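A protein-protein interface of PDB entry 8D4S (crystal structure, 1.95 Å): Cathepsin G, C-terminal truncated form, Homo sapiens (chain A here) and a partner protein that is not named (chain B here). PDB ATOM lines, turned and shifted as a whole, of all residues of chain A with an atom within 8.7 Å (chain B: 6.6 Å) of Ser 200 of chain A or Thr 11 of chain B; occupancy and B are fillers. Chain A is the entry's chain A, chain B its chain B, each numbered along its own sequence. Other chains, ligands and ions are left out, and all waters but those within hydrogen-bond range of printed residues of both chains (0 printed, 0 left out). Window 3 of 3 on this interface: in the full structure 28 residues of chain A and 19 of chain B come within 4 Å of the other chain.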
ATOM      1  N   ILE A   2      19.291  -1.066 -41.275  1.00  0.00           N
ATOM      2  CA  ILE A   2      17.844  -1.209 -41.360  1.00  0.00           C
ATOM      3  C   ILE A   2      17.408  -0.902 -42.787  1.00  0.00           C
ATOM      4  O   ILE A   2      17.836   0.100 -43.369  1.00  0.00           O
ATOM      5  CB  ILE A   2      17.147  -0.286 -40.346  1.00  0.00           C
ATOM      6  CG1 ILE A   2      17.417  -0.789 -38.925  1.00  0.00           C
ATOM      7  CG2 ILE A   2      15.636  -0.196 -40.620  1.00  0.00           C
ATOM      8  CD1 ILE A   2      17.115   0.228 -37.852  1.00  0.00           C
ATOM      9  N   ARG A  83      30.029  12.314 -23.662  1.00  0.00           N
ATOM     10  CA  ARG A  83      28.671  12.545 -23.176  1.00  0.00           C
ATOM     11  C   ARG A  83      27.770  13.046 -24.299  1.00  0.00           C
ATOM     12  O   ARG A  83      26.636  12.573 -24.452  1.00  0.00           O
ATOM     13  CB  ARG A  83      28.685  13.512 -21.981  1.00  0.00           C
ATOM     14  CG  ARG A  83      28.866  14.984 -22.321  1.00  0.00           C
ATOM     15  CD  ARG A  83      29.135  15.895 -21.115  1.00  0.00           C
ATOM     16  NE  ARG A  83      29.396  17.273 -21.545  1.00  0.00           N
ATOM     17  CZ  ARG A  83      30.607  17.818 -21.654  1.00  0.00           C
ATOM     18  NH1 ARG A  83      31.690  17.111 -21.351  1.00  0.00           N
ATOM     19  NH2 ARG A  83      30.739  19.078 -22.060  1.00  0.00           N
ATOM     20  N   ILE A  85      28.799  12.897 -27.599  1.00  0.00           N
ATOM     21  CA  ILE A  85      29.234  12.190 -28.808  1.00  0.00           C
ATOM     22  C   ILE A  85      29.721  13.193 -29.852  1.00  0.00           C
ATOM     23  O   ILE A  85      29.384  13.085 -31.031  1.00  0.00           O
ATOM     24  CB  ILE A  85      28.123  11.299 -29.395  1.00  0.00           C
ATOM     25  CG1 ILE A  85      27.332  10.592 -28.294  1.00  0.00           C
ATOM     26  CG2 ILE A  85      28.703  10.251 -30.341  1.00  0.00           C
ATOM     27  CD1 ILE A  85      26.214   9.722 -28.825  1.00  0.00           C
ATOM     28  N   SER A 131      17.134  -4.898 -37.295  1.00  0.00           N
ATOM     29  CA  SER A 131      15.897  -4.543 -36.618  1.00  0.00           C
ATOM     30  C   SER A 131      16.191  -4.620 -35.127  1.00  0.00           C
ATOM     31  O   SER A 131      17.309  -4.951 -34.716  1.00  0.00           O
ATOM     32  CB  SER A 131      14.748  -5.470 -37.016  1.00  0.00           C
ATOM     33  OG  SER A 131      14.811  -6.695 -36.305  1.00  0.00           O
ATOM     34  N   MET A 132      15.187  -4.315 -34.312  1.00  0.00           N
ATOM     35  CA  MET A 132      15.333  -4.512 -32.877  1.00  0.00           C
ATOM     36  C   MET A 132      15.274  -5.984 -32.468  1.00  0.00           C
ATOM     37  O   MET A 132      15.470  -6.287 -31.288  1.00  0.00           O
ATOM     38  CB  MET A 132      14.265  -3.707 -32.123  1.00  0.00           C
ATOM     39  CG  MET A 132      14.457  -2.197 -32.240  1.00  0.00           C
ATOM     40  SD  MET A 132      13.223  -1.238 -31.344  1.00  0.00           S
ATOM     41  CE  MET A 132      13.442  -1.873 -29.681  1.00  0.00           C
ATOM     42  N   PHE A 156      18.349  16.612 -32.089  1.00  0.00           N
ATOM     43  CA  PHE A 156      19.618  16.274 -31.437  1.00  0.00           C
ATOM     44  C   PHE A 156      20.249  17.556 -30.901  1.00  0.00           C
ATOM     45  O   PHE A 156      20.821  18.343 -31.656  1.00  0.00           O
ATOM     46  CB  PHE A 156      20.550  15.539 -32.401  1.00  0.00           C
ATOM     47  CG  PHE A 156      20.008  14.220 -32.864  1.00  0.00           C
ATOM     48  CD1 PHE A 156      19.507  13.300 -31.945  1.00  0.00           C
ATOM     49  CD2 PHE A 156      19.956  13.918 -34.211  1.00  0.00           C
ATOM     50  CE1 PHE A 156      18.992  12.098 -32.365  1.00  0.00           C
ATOM     51  CE2 PHE A 156      19.447  12.701 -34.637  1.00  0.00           C
ATOM     52  CZ  PHE A 156      18.976  11.790 -33.721  1.00  0.00           C
ATOM     53  N   ALA A 176      21.500   3.286 -40.581  1.00  0.00           N
ATOM     54  CA  ALA A 176      22.519   2.477 -39.932  1.00  0.00           C
ATOM     55  C   ALA A 176      22.083   2.244 -38.491  1.00  0.00           C
ATOM     56  O   ALA A 176      21.345   3.051 -37.915  1.00  0.00           O
ATOM     57  CB  ALA A 176      23.878   3.175 -39.997  1.00  0.00           C
ATOM     58  N   PHE A 177      22.497   1.122 -37.909  1.00  0.00           N
ATOM     59  CA  PHE A 177      21.935   0.740 -36.608  1.00  0.00           C
ATOM     60  C   PHE A 177      23.034   0.123 -35.743  1.00  0.00           C
ATOM     61  O   PHE A 177      24.231   0.370 -35.948  1.00  0.00           O
ATOM     62  CB  PHE A 177      20.709  -0.160 -36.827  1.00  0.00           C
ATOM     63  CG  PHE A 177      19.784  -0.225 -35.642  1.00  0.00           C
ATOM     64  CD1 PHE A 177      19.475   0.924 -34.919  1.00  0.00           C
ATOM     65  CD2 PHE A 177      19.224  -1.435 -35.251  1.00  0.00           C
ATOM     66  CE1 PHE A 177      18.617   0.867 -33.824  1.00  0.00           C
ATOM     67  CE2 PHE A 177      18.375  -1.506 -34.153  1.00  0.00           C
ATOM     68  CZ  PHE A 177      18.067  -0.351 -33.441  1.00  0.00           C
ATOM     69  N   LYS A 178      22.634  -0.664 -34.740  1.00  0.00           N
ATOM     70  CA  LYS A 178      23.558  -1.101 -33.691  1.00  0.00           C
ATOM     71  C   LYS A 178      24.578  -2.073 -34.264  1.00  0.00           C
ATOM     72  O   LYS A 178      24.208  -3.137 -34.755  1.00  0.00           O
ATOM     73  CB  LYS A 178      22.787  -1.757 -32.543  1.00  0.00           C
ATOM     74  CG  LYS A 178      21.670  -0.869 -31.951  1.00  0.00           C
ATOM     75  CD  LYS A 178      22.207   0.495 -31.546  1.00  0.00           C
ATOM     76  CE  LYS A 178      21.168   1.315 -30.749  1.00  0.00           C
ATOM     77  NZ  LYS A 178      21.612   2.740 -30.626  1.00  0.00           N
ATOM     78  N   TYR A 197      25.748   8.244 -34.352  1.00  0.00           N
ATOM     79  CA  TYR A 197      24.684   7.978 -33.393  1.00  0.00           C
ATOM     80  C   TYR A 197      23.317   8.263 -33.999  1.00  0.00           C
ATOM     81  O   TYR A 197      23.201   8.819 -35.090  1.00  0.00           O
ATOM     82  CB  TYR A 197      24.899   8.775 -32.103  1.00  0.00           C
ATOM     83  CG  TYR A 197      24.782  10.286 -32.197  1.00  0.00           C
ATOM     84  CD1 TYR A 197      23.552  10.916 -32.052  1.00  0.00           C
ATOM     85  CD2 TYR A 197      25.908  11.091 -32.370  1.00  0.00           C
ATOM     86  CE1 TYR A 197      23.435  12.303 -32.110  1.00  0.00           C
ATOM     87  CE2 TYR A 197      25.797  12.477 -32.419  1.00  0.00           C
ATOM     88  CZ  TYR A 197      24.558  13.070 -32.280  1.00  0.00           C
ATOM     89  OH  TYR A 197      24.437  14.436 -32.322  1.00  0.00           O
ATOM     90  N   GLY A 198      22.281   7.848 -33.278  1.00  0.00           N
ATOM     91  CA  GLY A 198      20.913   8.158 -33.654  1.00  0.00           C
ATOM     92  C   GLY A 198      19.955   8.047 -32.480  1.00  0.00           C
ATOM     93  O   GLY A 198      20.328   8.220 -31.313  1.00  0.00           O
ATOM     94  N   LYS A 199      18.701   7.760 -32.787  1.00  0.00           N
ATOM     95  CA  LYS A 199      17.726   7.380 -31.773  1.00  0.00           C
ATOM     96  C   LYS A 199      17.808   5.880 -31.525  1.00  0.00           C
ATOM     97  O   LYS A 199      18.178   5.111 -32.412  1.00  0.00           O
ATOM     98  CB  LYS A 199      16.313   7.741 -32.217  1.00  0.00           C
ATOM     99  CG  LYS A 199      16.078   9.227 -32.406  1.00  0.00           C
ATOM    100  CD  LYS A 199      16.255   9.939 -31.086  1.00  0.00           C
ATOM    101  CE  LYS A 199      15.557  11.286 -31.044  1.00  0.00           C
ATOM    102  NZ  LYS A 199      15.955  12.010 -29.804  1.00  0.00           N
ATOM    103  N   SER A 200      17.444   5.462 -30.309  1.00  0.00           N
ATOM    104  CA  SER A 200      17.497   4.037 -29.982  1.00  0.00           C
ATOM    105  C   SER A 200      16.547   3.210 -30.839  1.00  0.00           C
ATOM    106  O   SER A 200      16.784   2.008 -31.035  1.00  0.00           O
ATOM    107  CB  SER A 200      17.176   3.819 -28.500  1.00  0.00           C
ATOM    108  OG  SER A 200      15.908   4.363 -28.172  1.00  0.00           O
ATOM    109  N   SER A 201      15.477   3.826 -31.350  1.00  0.00           N
ATOM    110  CA  SER A 201      14.539   3.151 -32.241  1.00  0.00           C
ATOM    111  C   SER A 201      15.085   2.931 -33.647  1.00  0.00           C
ATOM    112  O   SER A 201      14.477   2.186 -34.421  1.00  0.00           O
ATOM    113  CB  SER A 201      13.256   3.970 -32.345  1.00  0.00           C
ATOM    114  OG  SER A 201      13.539   5.196 -32.994  1.00  0.00           O
ATOM    115  N   GLY A 202      16.188   3.572 -34.012  1.00  0.00           N
ATOM    116  CA  GLY A 202      16.658   3.491 -35.380  1.00  0.00           C
ATOM    117  C   GLY A 202      15.880   4.332 -36.367  1.00  0.00           C
ATOM    118  O   GLY A 202      16.207   4.315 -37.560  1.00  0.00           O
ATOM    119  N   VAL A 203      14.871   5.068 -35.918  1.00  0.00           N
ATOM    120  CA  VAL A 203      14.130   5.963 -36.815  1.00  0.00           C
ATOM    121  C   VAL A 203      15.030   7.136 -37.207  1.00  0.00           C
ATOM    122  O   VAL A 203      15.648   7.760 -36.328  1.00  0.00           O
ATOM    123  CB  VAL A 203      12.849   6.444 -36.134  1.00  0.00           C
ATOM    124  CG1 VAL A 203      12.127   7.490 -36.996  1.00  0.00           C
ATOM    125  CG2 VAL A 203      11.934   5.241 -35.828  1.00  0.00           C
ATOM    126  N   PRO A 205      16.150  11.016 -38.747  1.00  0.00           N
ATOM    127  CA  PRO A 205      17.549  11.165 -39.182  1.00  0.00           C
ATOM    128  C   PRO A 205      18.548  10.638 -38.168  1.00  0.00           C
ATOM    129  O   PRO A 205      18.236  10.478 -36.986  1.00  0.00           O
ATOM    130  CB  PRO A 205      17.719  12.685 -39.345  1.00  0.00           C
ATOM    131  CG  PRO A 205      16.360  13.279 -39.174  1.00  0.00           C
ATOM    132  CD  PRO A 205      15.552  12.311 -38.388  1.00  0.00           C
ATOM    133  N   THR B   9      21.855  -1.357 -24.678  1.00  0.00           N
ATOM    134  CA  THR B   9      21.854  -0.099 -25.419  1.00  0.00           C
ATOM    135  C   THR B   9      21.776   1.027 -24.406  1.00  0.00           C
ATOM    136  O   THR B   9      21.248   0.852 -23.299  1.00  0.00           O
ATOM    137  CB  THR B   9      20.666   0.020 -26.416  1.00  0.00           C
ATOM    138  OG1 THR B   9      19.430  -0.188 -25.717  1.00  0.00           O
ATOM    139  CG2 THR B   9      20.782  -0.998 -27.557  1.00  0.00           C
ATOM    140  N   ILE B  10      22.336   2.176 -24.764  1.00  0.00           N
ATOM    141  CA  ILE B  10      22.403   3.313 -23.851  1.00  0.00           C
ATOM    142  C   ILE B  10      21.890   4.541 -24.586  1.00  0.00           C
ATOM    143  O   ILE B  10      22.357   4.852 -25.685  1.00  0.00           O
ATOM    144  CB  ILE B  10      23.834   3.574 -23.346  1.00  0.00           C
ATOM    145  CG1 ILE B  10      24.357   2.380 -22.554  1.00  0.00           C
ATOM    146  CG2 ILE B  10      23.886   4.875 -22.529  1.00  0.00           C
ATOM    147  CD1 ILE B  10      25.815   2.518 -22.153  1.00  0.00           C
ATOM    148  N   THR B  11      20.944   5.239 -23.982  1.00  0.00           N
ATOM    149  CA  THR B  11      20.481   6.509 -24.515  1.00  0.00           C
ATOM    150  C   THR B  11      20.721   7.580 -23.471  1.00  0.00           C
ATOM    151  O   THR B  11      20.377   7.406 -22.296  1.00  0.00           O
ATOM    152  CB  THR B  11      19.006   6.451 -24.908  1.00  0.00           C
ATOM    153  OG1 THR B  11      18.841   5.489 -25.955  1.00  0.00           O
ATOM    154  CG2 THR B  11      18.532   7.815 -25.400  1.00  0.00           C
ATOM    155  N   VAL B  12      21.332   8.678 -23.889  1.00  0.00           N
ATOM    156  CA  VAL B  12      21.587   9.796 -23.002  1.00  0.00           C
ATOM    157  C   VAL B  12      21.188  11.057 -23.737  1.00  0.00           C
ATOM    158  O   VAL B  12      21.656  11.293 -24.856  1.00  0.00           O
ATOM    159  CB  VAL B  12      23.061   9.869 -22.576  1.00  0.00           C
ATOM    160  CG1 VAL B  12      23.268  11.087 -21.686  1.00  0.00           C
ATOM    161  CG2 VAL B  12      23.493   8.574 -21.889  1.00  0.00           C
ATOM    162  N   ASN B  13      20.317  11.855 -23.116  1.00  0.00           N
ATOM    163  CA  ASN B  13      19.833  13.100 -23.710  1.00  0.00           C
ATOM    164  C   ASN B  13      19.330  12.869 -25.129  1.00  0.00           C
ATOM    165  O   ASN B  13      19.581  13.663 -26.035  1.00  0.00           O
ATOM    166  CB  ASN B  13      20.915  14.176 -23.687  1.00  0.00           C
ATOM    167  CG  ASN B  13      21.134  14.749 -22.304  1.00  0.00           C
ATOM    168  OD1 ASN B  13      22.267  14.847 -21.829  1.00  0.00           O
ATOM    169  ND2 ASN B  13      20.044  15.137 -21.648  1.00  0.00           N
ATOM    170  N   GLY B  14      18.649  11.746 -25.327  1.00  0.00           N
ATOM    171  CA  GLY B  14      18.020  11.449 -26.597  1.00  0.00           C
ATOM    172  C   GLY B  14      18.918  10.908 -27.689  1.00  0.00           C
ATOM    173  O   GLY B  14      18.447  10.747 -28.820  1.00  0.00           O
ATOM    174  N   THR B  15      20.192  10.624 -27.408  1.00  0.00           N
ATOM    175  CA  THR B  15      21.109  10.106 -28.418  1.00  0.00           C
ATOM    176  C   THR B  15      21.668   8.759 -27.979  1.00  0.00           C
ATOM    177  O   THR B  15      21.923   8.532 -26.789  1.00  0.00           O
ATOM    178  CB  THR B  15      22.254  11.087 -28.681  1.00  0.00           C
ATOM    179  OG1 THR B  15      23.063  11.202 -27.503  1.00  0.00           O
ATOM    180  CG2 THR B  15      21.694  12.459 -29.036  1.00  0.00           C
ATOM    181  N   SER B  16      21.878   7.877 -28.947  1.00  0.00           N
ATOM    182  CA  SER B  16      22.303   6.510 -28.672  1.00  0.00           C
ATOM    183  C   SER B  16      23.354   6.126 -29.694  1.00  0.00           C
ATOM    184  O   SER B  16      23.098   6.215 -30.899  1.00  0.00           O
ATOM    185  CB  SER B  16      21.105   5.554 -28.735  1.00  0.00           C
ATOM    186  OG  SER B  16      21.491   4.220 -28.491  1.00  0.00           O
ATOM    187  N   GLN B  17      24.529   5.707 -29.221  1.00  0.00           N
ATOM    188  CA  GLN B  17      25.601   5.318 -30.132  1.00  0.00           C
ATOM    189  C   GLN B  17      25.184   4.085 -30.916  1.00  0.00           C
ATOM    190  O   GLN B  17      24.481   3.207 -30.403  1.00  0.00           O
ATOM    191  CB  GLN B  17      26.898   5.024 -29.363  1.00  0.00           C
ATOM    192  CG  GLN B  17      27.439   6.155 -28.480  1.00  0.00           C
ATOM    193  CD  GLN B  17      28.471   5.645 -27.482  1.00  0.00           C
ATOM    194  OE1 GLN B  17      28.552   4.442 -27.222  1.00  0.00           O
ATOM    195  NE2 GLN B  17      29.279   6.543 -26.947  1.00  0.00           N
ATOM    196  N   LEU B  44      27.753   2.444 -18.472  1.00  0.00           N
ATOM    197  CA  LEU B  44      27.384   3.854 -18.567  1.00  0.00           C
ATOM    198  C   LEU B  44      28.609   4.752 -18.456  1.00  0.00           C
ATOM    199  O   LEU B  44      28.725   5.757 -19.165  1.00  0.00           O
ATOM    200  CB  LEU B  44      26.389   4.217 -17.465  1.00  0.00           C
ATOM    201  CG  LEU B  44      24.932   4.544 -17.790  1.00  0.00           C
ATOM    202  CD1 LEU B  44      24.175   4.822 -16.489  1.00  0.00           C
ATOM    203  CD2 LEU B  44      24.853   5.730 -18.718  1.00  0.00           C
ATOM    204  N   ARG B  48      29.613   6.477 -21.981  1.00  0.00           N
ATOM    205  CA  ARG B  48      29.135   7.850 -22.062  1.00  0.00           C
ATOM    206  C   ARG B  48      29.668   8.723 -20.936  1.00  0.00           C
ATOM    207  O   ARG B  48      29.182   9.847 -20.762  1.00  0.00           O
ATOM    208  CB  ARG B  48      27.600   7.887 -22.094  1.00  0.00           C
ATOM    209  CG  ARG B  48      26.974   7.210 -23.320  1.00  0.00           C
ATOM    210  CD  ARG B  48      27.340   7.899 -24.650  1.00  0.00           C
ATOM    211  NE  ARG B  48      26.697   9.211 -24.797  1.00  0.00           N
ATOM    212  CZ  ARG B  48      25.483   9.392 -25.315  1.00  0.00           C
ATOM    213  NH1 ARG B  48      24.765   8.355 -25.719  1.00  0.00           N
ATOM    214  NH2 ARG B  48      24.979  10.606 -25.405  1.00  0.00           N
ATOM    215  N   ILE B  50      29.326   8.738 -17.777  1.00  0.00           N
ATOM    216  CA  ILE B  50      28.358   9.077 -16.741  1.00  0.00           C
ATOM    217  C   ILE B  50      28.595   8.164 -15.545  1.00  0.00           C
ATOM    218  O   ILE B  50      28.611   6.934 -15.686  1.00  0.00           O
ATOM    219  CB  ILE B  50      26.922   8.960 -17.273  1.00  0.00           C
ATOM    220  CG1 ILE B  50      26.664  10.071 -18.289  1.00  0.00           C
ATOM    221  CG2 ILE B  50      25.908   8.989 -16.148  1.00  0.00           C
ATOM    222  CD1 ILE B  50      25.347   9.947 -18.991  1.00  0.00           C
ATOM    223  N   SER B  96      18.245  -2.054 -21.558  1.00  0.00           N
ATOM    224  CA  SER B  96      18.292  -0.714 -22.123  1.00  0.00           C
ATOM    225  C   SER B  96      18.442   0.286 -20.989  1.00  0.00           C
ATOM    226  O   SER B  96      17.870   0.099 -19.916  1.00  0.00           O
ATOM    227  CB  SER B  96      17.044  -0.415 -22.943  1.00  0.00           C
ATOM    228  OG  SER B  96      15.899  -0.442 -22.118  1.00  0.00           O
ATOM    229  N   VAL B  97      19.242   1.322 -21.214  1.00  0.00           N
ATOM    230  CA  VAL B  97      19.507   2.348 -20.214  1.00  0.00           C
ATOM    231  C   VAL B  97      19.122   3.686 -20.814  1.00  0.00           C
ATOM    232  O   VAL B  97      19.435   3.963 -21.974  1.00  0.00           O
ATOM    233  CB  VAL B  97      20.989   2.383 -19.790  1.00  0.00           C
ATOM    234  CG1 VAL B  97      21.164   3.263 -18.558  1.00  0.00           C
ATOM    235  CG2 VAL B  97      21.519   0.978 -19.559  1.00  0.00           C
ATOM    236  N   ASN B  98      18.457   4.518 -20.025  1.00  0.00           N
ATOM    237  CA  ASN B  98      18.061   5.837 -20.499  1.00  0.00           C
ATOM    238  C   ASN B  98      18.311   6.855 -19.400  1.00  0.00           C
ATOM    239  O   ASN B  98      17.795   6.707 -18.288  1.00  0.00           O
ATOM    240  CB  ASN B  98      16.589   5.857 -20.919  1.00  0.00           C
ATOM    241  CG  ASN B  98      16.160   7.206 -21.415  1.00  0.00           C
ATOM    242  OD1 ASN B  98      16.465   7.585 -22.540  1.00  0.00           O
ATOM    243  ND2 ASN B  98      15.459   7.954 -20.572  1.00  0.00           N
ATOM    244  N   VAL B  99      19.092   7.885 -19.716  1.00  0.00           N
ATOM    245  CA  VAL B  99      19.381   8.981 -18.800  1.00  0.00           C
ATOM    246  C   VAL B  99      19.020  10.280 -19.492  1.00  0.00           C
ATOM    247  O   VAL B  99      19.372  10.485 -20.660  1.00  0.00           O
ATOM    248  CB  VAL B  99      20.864   9.003 -18.380  1.00  0.00           C
ATOM    249  CG1 VAL B  99      21.100  10.059 -17.319  1.00  0.00           C
ATOM    250  CG2 VAL B  99      21.310   7.624 -17.901  1.00  0.00           C
ATOM    251  N   ASP B 100      18.329  11.160 -18.773  1.00  0.00           N
ATOM    252  CA  ASP B 100      17.998  12.485 -19.298  1.00  0.00           C
ATOM    253  C   ASP B 100      18.762  13.580 -18.557  1.00  0.00           C
ATOM    254  O   ASP B 100      19.314  14.492 -19.175  1.00  0.00           O
ATOM    255  CB  ASP B 100      16.494  12.746 -19.202  1.00  0.00           C
ATOM    256  CG  ASP B 100      15.679  11.768 -20.021  1.00  0.00           C
ATOM    257  OD1 ASP B 100      16.276  11.017 -20.818  1.00  0.00           O
ATOM    258  OD2 ASP B 100      14.441  11.745 -19.863  1.00  0.00           O
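Of the printed residues of chain B, Phe 156 of chain A touches Gly 14 and Thr 15.
Printed residues of chain B within 4 Å of Gly 198 of chain A: Thr 15 and Ser 16.
Of the printed residues of chain B, Lys 199 of chain A touches Gly 14 (3.0 Å).
Of the printed residues of chain B, Ser 200 of chain A touches Thr 11 (3.5 Å) and Ser 16 (3.99 Å).
Of the printed residues of chain A, Thr 9 of chain B touches Lys 178 (3.96 Å).
Thr 11 of chain B touches one residue of chain A.
Printed residues of chain A within 4 Å of Gly 14 of chain B: Phe 156 and Lys 199.
The nearest residue of chain A that does not touch Thr 11 of chain B is Lys 199 of chain A (5.7 Å).
The nearest printed residue of chain B that does not touch Lys 178 of chain A is Ile 10 of chain B (5.4 Å).
Hydrophobic or aromatic side chains of chain A within 4 Å of the printed part of chain B: Ile 85, Phe 156 and Tyr 197.
Among the printed residues, merely in contact across the chains: Ile 85 of chain A with Thr 15 of chain B (3.7 Å), Ile 85 of chain A with Gln 17 of chain B (3.8 Å), Ile 85 of chain A with Arg 48 of chain B (3.6 Å), Phe 156 of chain A with Gly 14 of chain B (3.8 Å), Phe 156 of chain A with Thr 15 of chain B (3.7 Å), Lys 178 of chain A with Thr 9 of chain B (3.96 Å), Tyr 197 of chain A with Thr 15 of chain B (3.5 Å), Tyr 197 of chain A with Ser 16 of chain B (3.4 Å), Gly 198 of chain A with Thr 15 of chain B (3.5 Å), Ser 200 of chain A with Thr 11 of chain B (3.5 Å) and Ser 200 of chain A with Ser 16 of chain B (3.99 Å).
The backbone carbonyl oxygen of Arg 83 of chain A lies within hydrogen-bond range of the guanidinium group of Arg 48 of chain B, 2.7 Å away.
The side-chain amino group (NZ) of Lys 178 of chain A sits at hydrogen-bond distance from the backbone carbonyl oxygen (O) of Gln 17 of chain B (2.9 Å).
O of Gly 14 of chain B sits at hydrogen-bond distance from NZ of Lys 199 of chain A, at 3.0 Å.
The backbone carbonyl oxygen (O) of Gly 198 of chain A lies within hydrogen-bond range of the backbone NH (N) of Ser 16 of chain B (2.8 Å).
The side-chain amino group of Lys 178 of chain A is in hydrogen-bond range of the side-chain hydroxyl of Ser 16 of chain B.
The side-chain hydroxyl of Thr 15 of chain B lies within hydrogen-bond range of the guanidinium group of Arg 48 of chain B (2.9 Å).
O of Val 12 of chain B lies within hydrogen-bond range of NH2 of Arg 48 of chain B (3.4 Å).
The backbone carbonyl oxygen (O) of Ile 10 of chain B is in hydrogen-bond range of the side-chain hydroxyl (OG) of Ser 16 of chain B.
The backbone NH (N) of Val 97 of chain B sits at hydrogen-bond distance from the backbone carbonyl oxygen (O) of Thr 9 of chain B, 2.9 Å away.
The backbone carbonyl oxygen (O) of Thr 11 of chain B lies within hydrogen-bond range of the backbone NH (N) of Val 99 of chain B (2.9 Å).
O of Val 97 of chain B lies within hydrogen-bond range of N of Thr 11 of chain B, 2.8 Å away.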
